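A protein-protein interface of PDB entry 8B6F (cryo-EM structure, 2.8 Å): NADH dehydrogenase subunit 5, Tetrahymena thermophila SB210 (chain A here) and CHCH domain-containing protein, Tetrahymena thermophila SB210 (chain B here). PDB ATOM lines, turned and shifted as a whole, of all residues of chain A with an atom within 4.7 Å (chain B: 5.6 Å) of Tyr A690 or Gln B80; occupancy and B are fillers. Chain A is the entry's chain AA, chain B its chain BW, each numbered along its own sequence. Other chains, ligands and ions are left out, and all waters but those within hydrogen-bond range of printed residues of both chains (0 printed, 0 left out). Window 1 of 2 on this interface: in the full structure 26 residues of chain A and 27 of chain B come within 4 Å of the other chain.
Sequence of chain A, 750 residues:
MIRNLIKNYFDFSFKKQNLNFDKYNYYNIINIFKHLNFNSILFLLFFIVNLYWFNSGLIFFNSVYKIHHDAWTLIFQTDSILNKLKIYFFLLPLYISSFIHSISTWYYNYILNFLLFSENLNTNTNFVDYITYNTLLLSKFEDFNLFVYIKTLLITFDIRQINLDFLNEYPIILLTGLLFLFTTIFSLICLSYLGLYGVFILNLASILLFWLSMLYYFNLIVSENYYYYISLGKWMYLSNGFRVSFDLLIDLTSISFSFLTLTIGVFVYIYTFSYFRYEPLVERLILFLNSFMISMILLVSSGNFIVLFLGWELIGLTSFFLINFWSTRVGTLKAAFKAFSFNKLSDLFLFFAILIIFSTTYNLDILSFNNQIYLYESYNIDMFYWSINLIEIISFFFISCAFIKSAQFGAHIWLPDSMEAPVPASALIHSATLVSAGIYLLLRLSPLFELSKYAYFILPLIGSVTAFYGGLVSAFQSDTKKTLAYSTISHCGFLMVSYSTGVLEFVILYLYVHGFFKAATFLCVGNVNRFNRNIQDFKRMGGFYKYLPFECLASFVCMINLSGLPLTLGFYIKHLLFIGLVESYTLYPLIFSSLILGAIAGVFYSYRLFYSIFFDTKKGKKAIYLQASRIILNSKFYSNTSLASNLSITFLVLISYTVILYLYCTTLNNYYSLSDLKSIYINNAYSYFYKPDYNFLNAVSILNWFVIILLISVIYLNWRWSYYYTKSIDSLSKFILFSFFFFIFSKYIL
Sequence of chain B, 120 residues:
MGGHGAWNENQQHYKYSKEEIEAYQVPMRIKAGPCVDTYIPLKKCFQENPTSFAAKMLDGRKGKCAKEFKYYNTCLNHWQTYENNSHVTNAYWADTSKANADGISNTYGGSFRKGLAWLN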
ATOM      1  N   THR A 667      21.072  25.463  13.982  1.00  0.00           N
ATOM      2  CA  THR A 667      20.524  24.428  14.855  1.00  0.00           C
ATOM      3  C   THR A 667      21.070  24.510  16.277  1.00  0.00           C
ATOM      4  O   THR A 667      20.300  24.597  17.238  1.00  0.00           O
ATOM      5  CB  THR A 667      20.804  23.040  14.263  1.00  0.00           C
ATOM      6  OG1 THR A 667      22.214  22.868  14.077  1.00  0.00           O
ATOM      7  CG2 THR A 667      20.103  22.876  12.929  1.00  0.00           C
ATOM      8  N   LEU A 668      22.391  24.480  16.430  1.00  0.00           N
ATOM      9  CA  LEU A 668      23.013  24.347  17.742  1.00  0.00           C
ATOM     10  C   LEU A 668      23.128  25.662  18.501  1.00  0.00           C
ATOM     11  O   LEU A 668      23.583  25.651  19.649  1.00  0.00           O
ATOM     12  CB  LEU A 668      24.402  23.726  17.588  1.00  0.00           C
ATOM     13  CG  LEU A 668      24.449  22.378  16.865  1.00  0.00           C
ATOM     14  CD1 LEU A 668      25.887  21.912  16.721  1.00  0.00           C
ATOM     15  CD2 LEU A 668      23.615  21.334  17.593  1.00  0.00           C
ATOM     16  N   ASN A 669      22.741  26.784  17.907  1.00  0.00           N
ATOM     17  CA  ASN A 669      22.841  28.059  18.596  1.00  0.00           C
ATOM     18  C   ASN A 669      21.750  28.178  19.660  1.00  0.00           C
ATOM     19  O   ASN A 669      20.762  27.438  19.660  1.00  0.00           O
ATOM     20  CB  ASN A 669      22.739  29.212  17.597  1.00  0.00           C
ATOM     21  CG  ASN A 669      23.057  30.554  18.217  1.00  0.00           C
ATOM     22  OD1 ASN A 669      23.693  30.630  19.266  1.00  0.00           O
ATOM     23  ND2 ASN A 669      22.612  31.623  17.572  1.00  0.00           N
ATOM     24  N   ASN A 670      21.942  29.125  20.581  1.00  0.00           N
ATOM     25  CA  ASN A 670      20.948  29.347  21.628  1.00  0.00           C
ATOM     26  C   ASN A 670      19.605  29.746  21.031  1.00  0.00           C
ATOM     27  O   ASN A 670      18.553  29.286  21.487  1.00  0.00           O
ATOM     28  CB  ASN A 670      21.434  30.415  22.606  1.00  0.00           C
ATOM     29  CG  ASN A 670      22.602  29.944  23.450  1.00  0.00           C
ATOM     30  OD1 ASN A 670      23.670  30.555  23.444  1.00  0.00           O
ATOM     31  ND2 ASN A 670      22.402  28.858  24.188  1.00  0.00           N
ATOM     32  N   ASN A 684      13.579  15.452  23.548  1.00  0.00           N
ATOM     33  CA  ASN A 684      14.182  15.986  24.763  1.00  0.00           C
ATOM     34  C   ASN A 684      15.706  15.923  24.722  1.00  0.00           C
ATOM     35  O   ASN A 684      16.354  16.266  25.716  1.00  0.00           O
ATOM     36  CB  ASN A 684      13.683  15.254  26.019  1.00  0.00           C
ATOM     37  CG  ASN A 684      14.153  15.898  27.301  1.00  0.00           C
ATOM     38  OD1 ASN A 684      14.447  17.091  27.336  1.00  0.00           O
ATOM     39  ND2 ASN A 684      14.240  15.105  28.364  1.00  0.00           N
ATOM     40  N   TYR A 686      17.835  17.791  23.253  1.00  0.00           N
ATOM     41  CA  TYR A 686      18.475  19.098  23.345  1.00  0.00           C
ATOM     42  C   TYR A 686      18.711  19.529  24.784  1.00  0.00           C
ATOM     43  O   TYR A 686      19.484  20.463  25.020  1.00  0.00           O
ATOM     44  CB  TYR A 686      17.629  20.151  22.628  1.00  0.00           C
ATOM     45  CG  TYR A 686      18.084  20.454  21.218  1.00  0.00           C
ATOM     46  CD1 TYR A 686      19.025  21.444  20.971  1.00  0.00           C
ATOM     47  CD2 TYR A 686      17.564  19.759  20.136  1.00  0.00           C
ATOM     48  CE1 TYR A 686      19.441  21.730  19.686  1.00  0.00           C
ATOM     49  CE2 TYR A 686      17.974  20.037  18.847  1.00  0.00           C
ATOM     50  CZ  TYR A 686      18.912  21.024  18.629  1.00  0.00           C
ATOM     51  OH  TYR A 686      19.322  21.304  17.350  1.00  0.00           O
ATOM     52  N   SER A 687      18.065  18.874  25.750  1.00  0.00           N
ATOM     53  CA  SER A 687      18.268  19.234  27.148  1.00  0.00           C
ATOM     54  C   SER A 687      19.705  18.971  27.578  1.00  0.00           C
ATOM     55  O   SER A 687      20.284  19.748  28.344  1.00  0.00           O
ATOM     56  CB  SER A 687      17.288  18.470  28.036  1.00  0.00           C
ATOM     57  OG  SER A 687      17.531  17.077  27.984  1.00  0.00           O
ATOM     58  N   TYR A 688      20.292  17.872  27.110  1.00  0.00           N
ATOM     59  CA  TYR A 688      21.672  17.545  27.442  1.00  0.00           C
ATOM     60  C   TYR A 688      22.681  18.275  26.567  1.00  0.00           C
ATOM     61  O   TYR A 688      23.886  18.130  26.788  1.00  0.00           O
ATOM     62  CB  TYR A 688      21.894  16.035  27.346  1.00  0.00           C
ATOM     63  CG  TYR A 688      21.179  15.279  28.434  1.00  0.00           C
ATOM     64  CD1 TYR A 688      19.867  14.859  28.269  1.00  0.00           C
ATOM     65  CD2 TYR A 688      21.809  15.007  29.639  1.00  0.00           C
ATOM     66  CE1 TYR A 688      19.206  14.178  29.268  1.00  0.00           C
ATOM     67  CE2 TYR A 688      21.159  14.329  30.645  1.00  0.00           C
ATOM     68  CZ  TYR A 688      19.857  13.918  30.454  1.00  0.00           C
ATOM     69  OH  TYR A 688      19.214  13.241  31.460  1.00  0.00           O
ATOM     70  N   PHE A 689      22.225  19.042  25.580  1.00  0.00           N
ATOM     71  CA  PHE A 689      23.099  19.947  24.851  1.00  0.00           C
ATOM     72  C   PHE A 689      23.070  21.359  25.411  1.00  0.00           C
ATOM     73  O   PHE A 689      24.084  22.061  25.350  1.00  0.00           O
ATOM     74  CB  PHE A 689      22.708  19.982  23.369  1.00  0.00           C
ATOM     75  CG  PHE A 689      23.470  20.995  22.569  1.00  0.00           C
ATOM     76  CD1 PHE A 689      24.778  20.749  22.187  1.00  0.00           C
ATOM     77  CD2 PHE A 689      22.879  22.187  22.190  1.00  0.00           C
ATOM     78  CE1 PHE A 689      25.484  21.675  21.450  1.00  0.00           C
ATOM     79  CE2 PHE A 689      23.579  23.119  21.452  1.00  0.00           C
ATOM     80  CZ  PHE A 689      24.883  22.861  21.080  1.00  0.00           C
ATOM     81  N   TYR A 690      21.934  21.788  25.962  1.00  0.00           N
ATOM     82  CA  TYR A 690      21.801  23.118  26.541  1.00  0.00           C
ATOM     83  C   TYR A 690      22.244  23.153  27.999  1.00  0.00           C
ATOM     84  O   TYR A 690      23.029  24.022  28.390  1.00  0.00           O
ATOM     85  CB  TYR A 690      20.349  23.597  26.426  1.00  0.00           C
ATOM     86  CG  TYR A 690      19.913  23.956  25.022  1.00  0.00           C
ATOM     87  CD1 TYR A 690      20.758  24.650  24.163  1.00  0.00           C
ATOM     88  CD2 TYR A 690      18.657  23.598  24.556  1.00  0.00           C
ATOM     89  CE1 TYR A 690      20.361  24.977  22.884  1.00  0.00           C
ATOM     90  CE2 TYR A 690      18.250  23.922  23.278  1.00  0.00           C
ATOM     91  CZ  TYR A 690      19.107  24.611  22.447  1.00  0.00           C
ATOM     92  OH  TYR A 690      18.705  24.935  21.173  1.00  0.00           O
ATOM     93  N   LYS A 691      21.754  22.218  28.812  1.00  0.00           N
ATOM     94  CA  LYS A 691      22.053  22.167  30.242  1.00  0.00           C
ATOM     95  C   LYS A 691      22.488  20.758  30.619  1.00  0.00           C
ATOM     96  O   LYS A 691      21.772  20.038  31.325  1.00  0.00           O
ATOM     97  CB  LYS A 691      20.840  22.596  31.069  1.00  0.00           C
ATOM     98  CG  LYS A 691      20.523  24.080  30.984  1.00  0.00           C
ATOM     99  CD  LYS A 691      21.551  24.908  31.738  1.00  0.00           C
ATOM    100  CE  LYS A 691      21.205  26.383  31.697  1.00  0.00           C
ATOM    101  NZ  LYS A 691      22.178  27.198  32.476  1.00  0.00           N
ATOM    102  N   PRO A 692      23.661  20.327  30.160  1.00  0.00           N
ATOM    103  CA  PRO A 692      24.164  19.010  30.560  1.00  0.00           C
ATOM    104  C   PRO A 692      24.496  18.971  32.043  1.00  0.00           C
ATOM    105  O   PRO A 692      24.854  19.981  32.653  1.00  0.00           O
ATOM    106  CB  PRO A 692      25.418  18.831  29.698  1.00  0.00           C
ATOM    107  CG  PRO A 692      25.858  20.217  29.384  1.00  0.00           C
ATOM    108  CD  PRO A 692      24.604  21.037  29.280  1.00  0.00           C
ATOM    109  N   CYS B  75      14.079  31.734  29.989  1.00  0.00           N
ATOM    110  CA  CYS B  75      13.050  30.722  29.786  1.00  0.00           C
ATOM    111  C   CYS B  75      13.660  29.424  29.281  1.00  0.00           C
ATOM    112  O   CYS B  75      13.268  28.332  29.709  1.00  0.00           O
ATOM    113  CB  CYS B  75      11.989  31.233  28.812  1.00  0.00           C
ATOM    114  SG  CYS B  75      10.523  30.183  28.734  1.00  0.00           S
ATOM    115  N   LEU B  76      14.628  29.522  28.368  1.00  0.00           N
ATOM    116  CA  LEU B  76      15.278  28.327  27.842  1.00  0.00           C
ATOM    117  C   LEU B  76      16.024  27.580  28.938  1.00  0.00           C
ATOM    118  O   LEU B  76      15.955  26.348  29.015  1.00  0.00           O
ATOM    119  CB  LEU B  76      16.224  28.707  26.702  1.00  0.00           C
ATOM    120  CG  LEU B  76      16.984  27.560  26.032  1.00  0.00           C
ATOM    121  CD1 LEU B  76      16.026  26.629  25.304  1.00  0.00           C
ATOM    122  CD2 LEU B  76      18.032  28.106  25.079  1.00  0.00           C
ATOM    123  N   ASN B  77      16.747  28.303  29.796  1.00  0.00           N
ATOM    124  CA  ASN B  77      17.447  27.648  30.896  1.00  0.00           C
ATOM    125  C   ASN B  77      16.472  26.887  31.787  1.00  0.00           C
ATOM    126  O   ASN B  77      16.692  25.715  32.107  1.00  0.00           O
ATOM    127  CB  ASN B  77      18.223  28.680  31.713  1.00  0.00           C
ATOM    128  CG  ASN B  77      19.399  29.258  30.955  1.00  0.00           C
ATOM    129  OD1 ASN B  77      19.914  28.641  30.025  1.00  0.00           O
ATOM    130  ND2 ASN B  77      19.830  30.449  31.350  1.00  0.00           N
ATOM    131  N   HIS B  78      15.386  27.543  32.202  1.00  0.00           N
ATOM    132  CA  HIS B  78      14.418  26.877  33.066  1.00  0.00           C
ATOM    133  C   HIS B  78      13.784  25.686  32.364  1.00  0.00           C
ATOM    134  O   HIS B  78      13.611  24.620  32.965  1.00  0.00           O
ATOM    135  CB  HIS B  78      13.346  27.869  33.513  1.00  0.00           C
ATOM    136  CG  HIS B  78      13.789  28.773  34.620  1.00  0.00           C
ATOM    137  ND1 HIS B  78      14.652  29.829  34.418  1.00  0.00           N
ATOM    138  CD2 HIS B  78      13.497  28.773  35.940  1.00  0.00           C
ATOM    139  CE1 HIS B  78      14.868  30.443  35.566  1.00  0.00           C
ATOM    140  NE2 HIS B  78      14.180  29.822  36.508  1.00  0.00           N
ATOM    141  N   TRP B  79      13.430  25.849  31.089  1.00  0.00           N
ATOM    142  CA  TRP B  79      12.796  24.766  30.345  1.00  0.00           C
ATOM    143  C   TRP B  79      13.695  23.537  30.291  1.00  0.00           C
ATOM    144  O   TRP B  79      13.262  22.422  30.603  1.00  0.00           O
ATOM    145  CB  TRP B  79      12.451  25.255  28.938  1.00  0.00           C
ATOM    146  CG  TRP B  79      11.965  24.194  28.003  1.00  0.00           C
ATOM    147  CD1 TRP B  79      11.326  23.034  28.329  1.00  0.00           C
ATOM    148  CD2 TRP B  79      12.079  24.201  26.576  1.00  0.00           C
ATOM    149  NE1 TRP B  79      11.037  22.319  27.193  1.00  0.00           N
ATOM    150  CE2 TRP B  79      11.489  23.015  26.103  1.00  0.00           C
ATOM    151  CE3 TRP B  79      12.625  25.100  25.653  1.00  0.00           C
ATOM    152  CZ2 TRP B  79      11.428  22.702  24.747  1.00  0.00           C
ATOM    153  CZ3 TRP B  79      12.564  24.788  24.307  1.00  0.00           C
ATOM    154  CH2 TRP B  79      11.969  23.598  23.865  1.00  0.00           C
ATOM    155  N   GLN B  80      14.953  23.721  29.889  1.00  0.00           N
ATOM    156  CA  GLN B  80      15.855  22.582  29.756  1.00  0.00           C
ATOM    157  C   GLN B  80      16.191  21.975  31.112  1.00  0.00           C
ATOM    158  O   GLN B  80      16.296  20.750  31.240  1.00  0.00           O
ATOM    159  CB  GLN B  80      17.127  23.003  29.023  1.00  0.00           C
ATOM    160  CG  GLN B  80      16.873  23.582  27.643  1.00  0.00           C
ATOM    161  CD  GLN B  80      16.163  22.611  26.720  1.00  0.00           C
ATOM    162  OE1 GLN B  80      16.062  21.422  27.007  1.00  0.00           O
ATOM    163  NE2 GLN B  80      15.667  23.120  25.599  1.00  0.00           N
ATOM    164  N   THR B  81      16.372  22.811  32.137  1.00  0.00           N
ATOM    165  CA  THR B  81      16.663  22.287  33.467  1.00  0.00           C
ATOM    166  C   THR B  81      15.521  21.421  33.979  1.00  0.00           C
ATOM    167  O   THR B  81      15.754  20.356  34.564  1.00  0.00           O
ATOM    168  CB  THR B  81      16.936  23.436  34.437  1.00  0.00           C
ATOM    169  OG1 THR B  81      18.068  24.189  33.986  1.00  0.00           O
ATOM    170  CG2 THR B  81      17.214  22.905  35.835  1.00  0.00           C
ATOM    171  N   TYR B  82      14.277  21.860  33.779  1.00  0.00           N
ATOM    172  CA  TYR B  82      13.141  21.064  34.226  1.00  0.00           C
ATOM    173  C   TYR B  82      12.937  19.836  33.351  1.00  0.00           C
ATOM    174  O   TYR B  82      12.430  18.817  33.830  1.00  0.00           O
ATOM    175  CB  TYR B  82      11.871  21.918  34.243  1.00  0.00           C
ATOM    176  CG  TYR B  82      11.934  23.095  35.192  1.00  0.00           C
ATOM    177  CD1 TYR B  82      12.706  23.046  36.345  1.00  0.00           C
ATOM    178  CD2 TYR B  82      11.224  24.257  34.931  1.00  0.00           C
ATOM    179  CE1 TYR B  82      12.768  24.117  37.208  1.00  0.00           C
ATOM    180  CE2 TYR B  82      11.279  25.336  35.790  1.00  0.00           C
ATOM    181  CZ  TYR B  82      12.055  25.259  36.927  1.00  0.00           C
ATOM    182  OH  TYR B  82      12.115  26.329  37.788  1.00  0.00           O
ATOM    183  N   GLU B  83      13.319  19.907  32.076  1.00  0.00           N
ATOM    184  CA  GLU B  83      13.165  18.745  31.209  1.00  0.00           C
ATOM    185  C   GLU B  83      14.122  17.623  31.597  1.00  0.00           C
ATOM    186  O   GLU B  83      13.719  16.456  31.654  1.00  0.00           O
ATOM    187  CB  GLU B  83      13.384  19.154  29.752  1.00  0.00           C
ATOM    188  CG  GLU B  83      12.194  19.857  29.120  1.00  0.00           C
ATOM    189  CD  GLU B  83      10.999  18.940  28.952  1.00  0.00           C
ATOM    190  OE1 GLU B  83      11.135  17.728  29.217  1.00  0.00           O
ATOM    191  OE2 GLU B  83       9.921  19.431  28.557  1.00  0.00           O
ATOM    192  N   ASN B  84      15.387  17.946  31.861  1.00  0.00           N
ATOM    193  CA  ASN B  84      16.377  16.927  32.191  1.00  0.00           C
ATOM    194  C   ASN B  84      16.552  16.722  33.692  1.00  0.00           C
ATOM    195  O   ASN B  84      17.349  15.867  34.091  1.00  0.00           O
ATOM    196  CB  ASN B  84      17.734  17.269  31.562  1.00  0.00           C
ATOM    197  CG  ASN B  84      18.309  18.568  32.075  1.00  0.00           C
ATOM    198  OD1 ASN B  84      17.763  19.188  32.985  1.00  0.00           O
ATOM    199  ND2 ASN B  84      19.429  18.984  31.498  1.00  0.00           N
ATOM    200  N   ASN B  85      15.829  17.467  34.529  1.00  0.00           N
ATOM    201  CA  ASN B  85      15.944  17.341  35.983  1.00  0.00           C
ATOM    202  C   ASN B  85      17.387  17.528  36.444  1.00  0.00           C
ATOM    203  O   ASN B  85      17.850  16.868  37.376  1.00  0.00           O
ATOM    204  CB  ASN B  85      15.401  15.996  36.460  1.00  0.00           C
ATOM    205  CG  ASN B  85      13.915  15.860  36.239  1.00  0.00           C
ATOM    206  OD1 ASN B  85      13.299  16.682  35.565  1.00  0.00           O
ATOM    207  ND2 ASN B  85      13.330  14.817  36.805  1.00  0.00           N
ATOM    208  N   SER B  86      18.105  18.445  35.795  1.00  0.00           N
ATOM    209  CA  SER B  86      19.517  18.630  36.114  1.00  0.00           C
ATOM    210  C   SER B  86      19.710  19.338  37.449  1.00  0.00           C
ATOM    211  O   SER B  86      20.742  19.146  38.102  1.00  0.00           O
ATOM    212  CB  SER B  86      20.214  19.406  34.996  1.00  0.00           C
ATOM    213  OG  SER B  86      19.671  20.706  34.854  1.00  0.00           O
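N of Ser A687 lies close to OE1 of Gln B80 (3.5 Å). The side-chain amide nitrogen (ND2) of Asn B84 lies within hydrogen-bond range of the backbone carbonyl oxygen (O) of Ser A687, 3.4 Å away. ND2 of Asn B84 sits at hydrogen-bond distance from O of Lys A691, 2.6 Å away.
The side-chain amide oxygen (OD1) of Asn B84 lies within hydrogen-bond range of the backbone NH (N) of Ser B86, 2.9 Å away. The backbone carbonyl oxygen of Asn B77 sits at hydrogen-bond distance from the side-chain hydroxyl of Thr B81 (2.8 Å). The backbone carbonyl oxygen (O) of Thr B81 is in hydrogen-bond range of the backbone NH (N) of Ser B86 (3.3 Å). O of Thr A667 is in hydrogen-bond range of OH of Tyr A686 (3.4 Å). O of Gln B80 lies close to OD1 of Asn B84 (2.8 Å). The backbone carbonyl oxygen (O) of Thr B81 sits close to the side-chain amide oxygen (OD1) of Asn B84.
Among the printed residues, pairs that only touch across the chains: Lys A691 with Asn B77 (3.1 Å), Tyr A690 with Gln B80 (3.2 Å), Asn A684 with Glu B83 (3.4 Å), Asn A670 with Leu B76 (3.8 Å), Lys A691 with Thr B81 (3.9 Å) and Tyr A686 with Gln B80 (3.9 Å).
Printed residues of chain B within 4 Å of Tyr A686: Gln B80. Of chain B, only Gln B80 comes within 4 Å of Tyr A690. Printed residues of chain A within 4 Å of Glu B83: Asn A684. The nearest residue of chain B that does not touch Tyr A690 is Leu B76 (4.05 Å). The nearest residue of chain A that does not touch Gln B80 is Lys A691 (4.1 Å). The nearest printed residue of chain A that does not touch Thr B81 is Ser A687 (6.0 Å).
Of the 12 printed residues of chain B, 6 touch a printed residue of chain A. Printed residues of chain B that touch a printed residue of chain A: Leu B76, Asn B77, Gln B80, Thr B81, Glu B83 and Asn B84. Hydrophobic or aromatic side chains of chain B within 4 Å of the printed part of chain A: Leu B76. Printed residues of chain A that touch a printed residue of chain B: Asn A670, Asn A684, Tyr A686, Ser A687, Tyr A690 and Lys A691. Hydrophobic or aromatic side chains of chain A within 4 Å of the printed part of chain B: Tyr A690. Among the printed residues, 9 pairs touch across the chains. Among the printed residues, no Asp or Glu carboxylate lies within 4 Å of a Lys or Arg side-chain nitrogen of the other chain.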
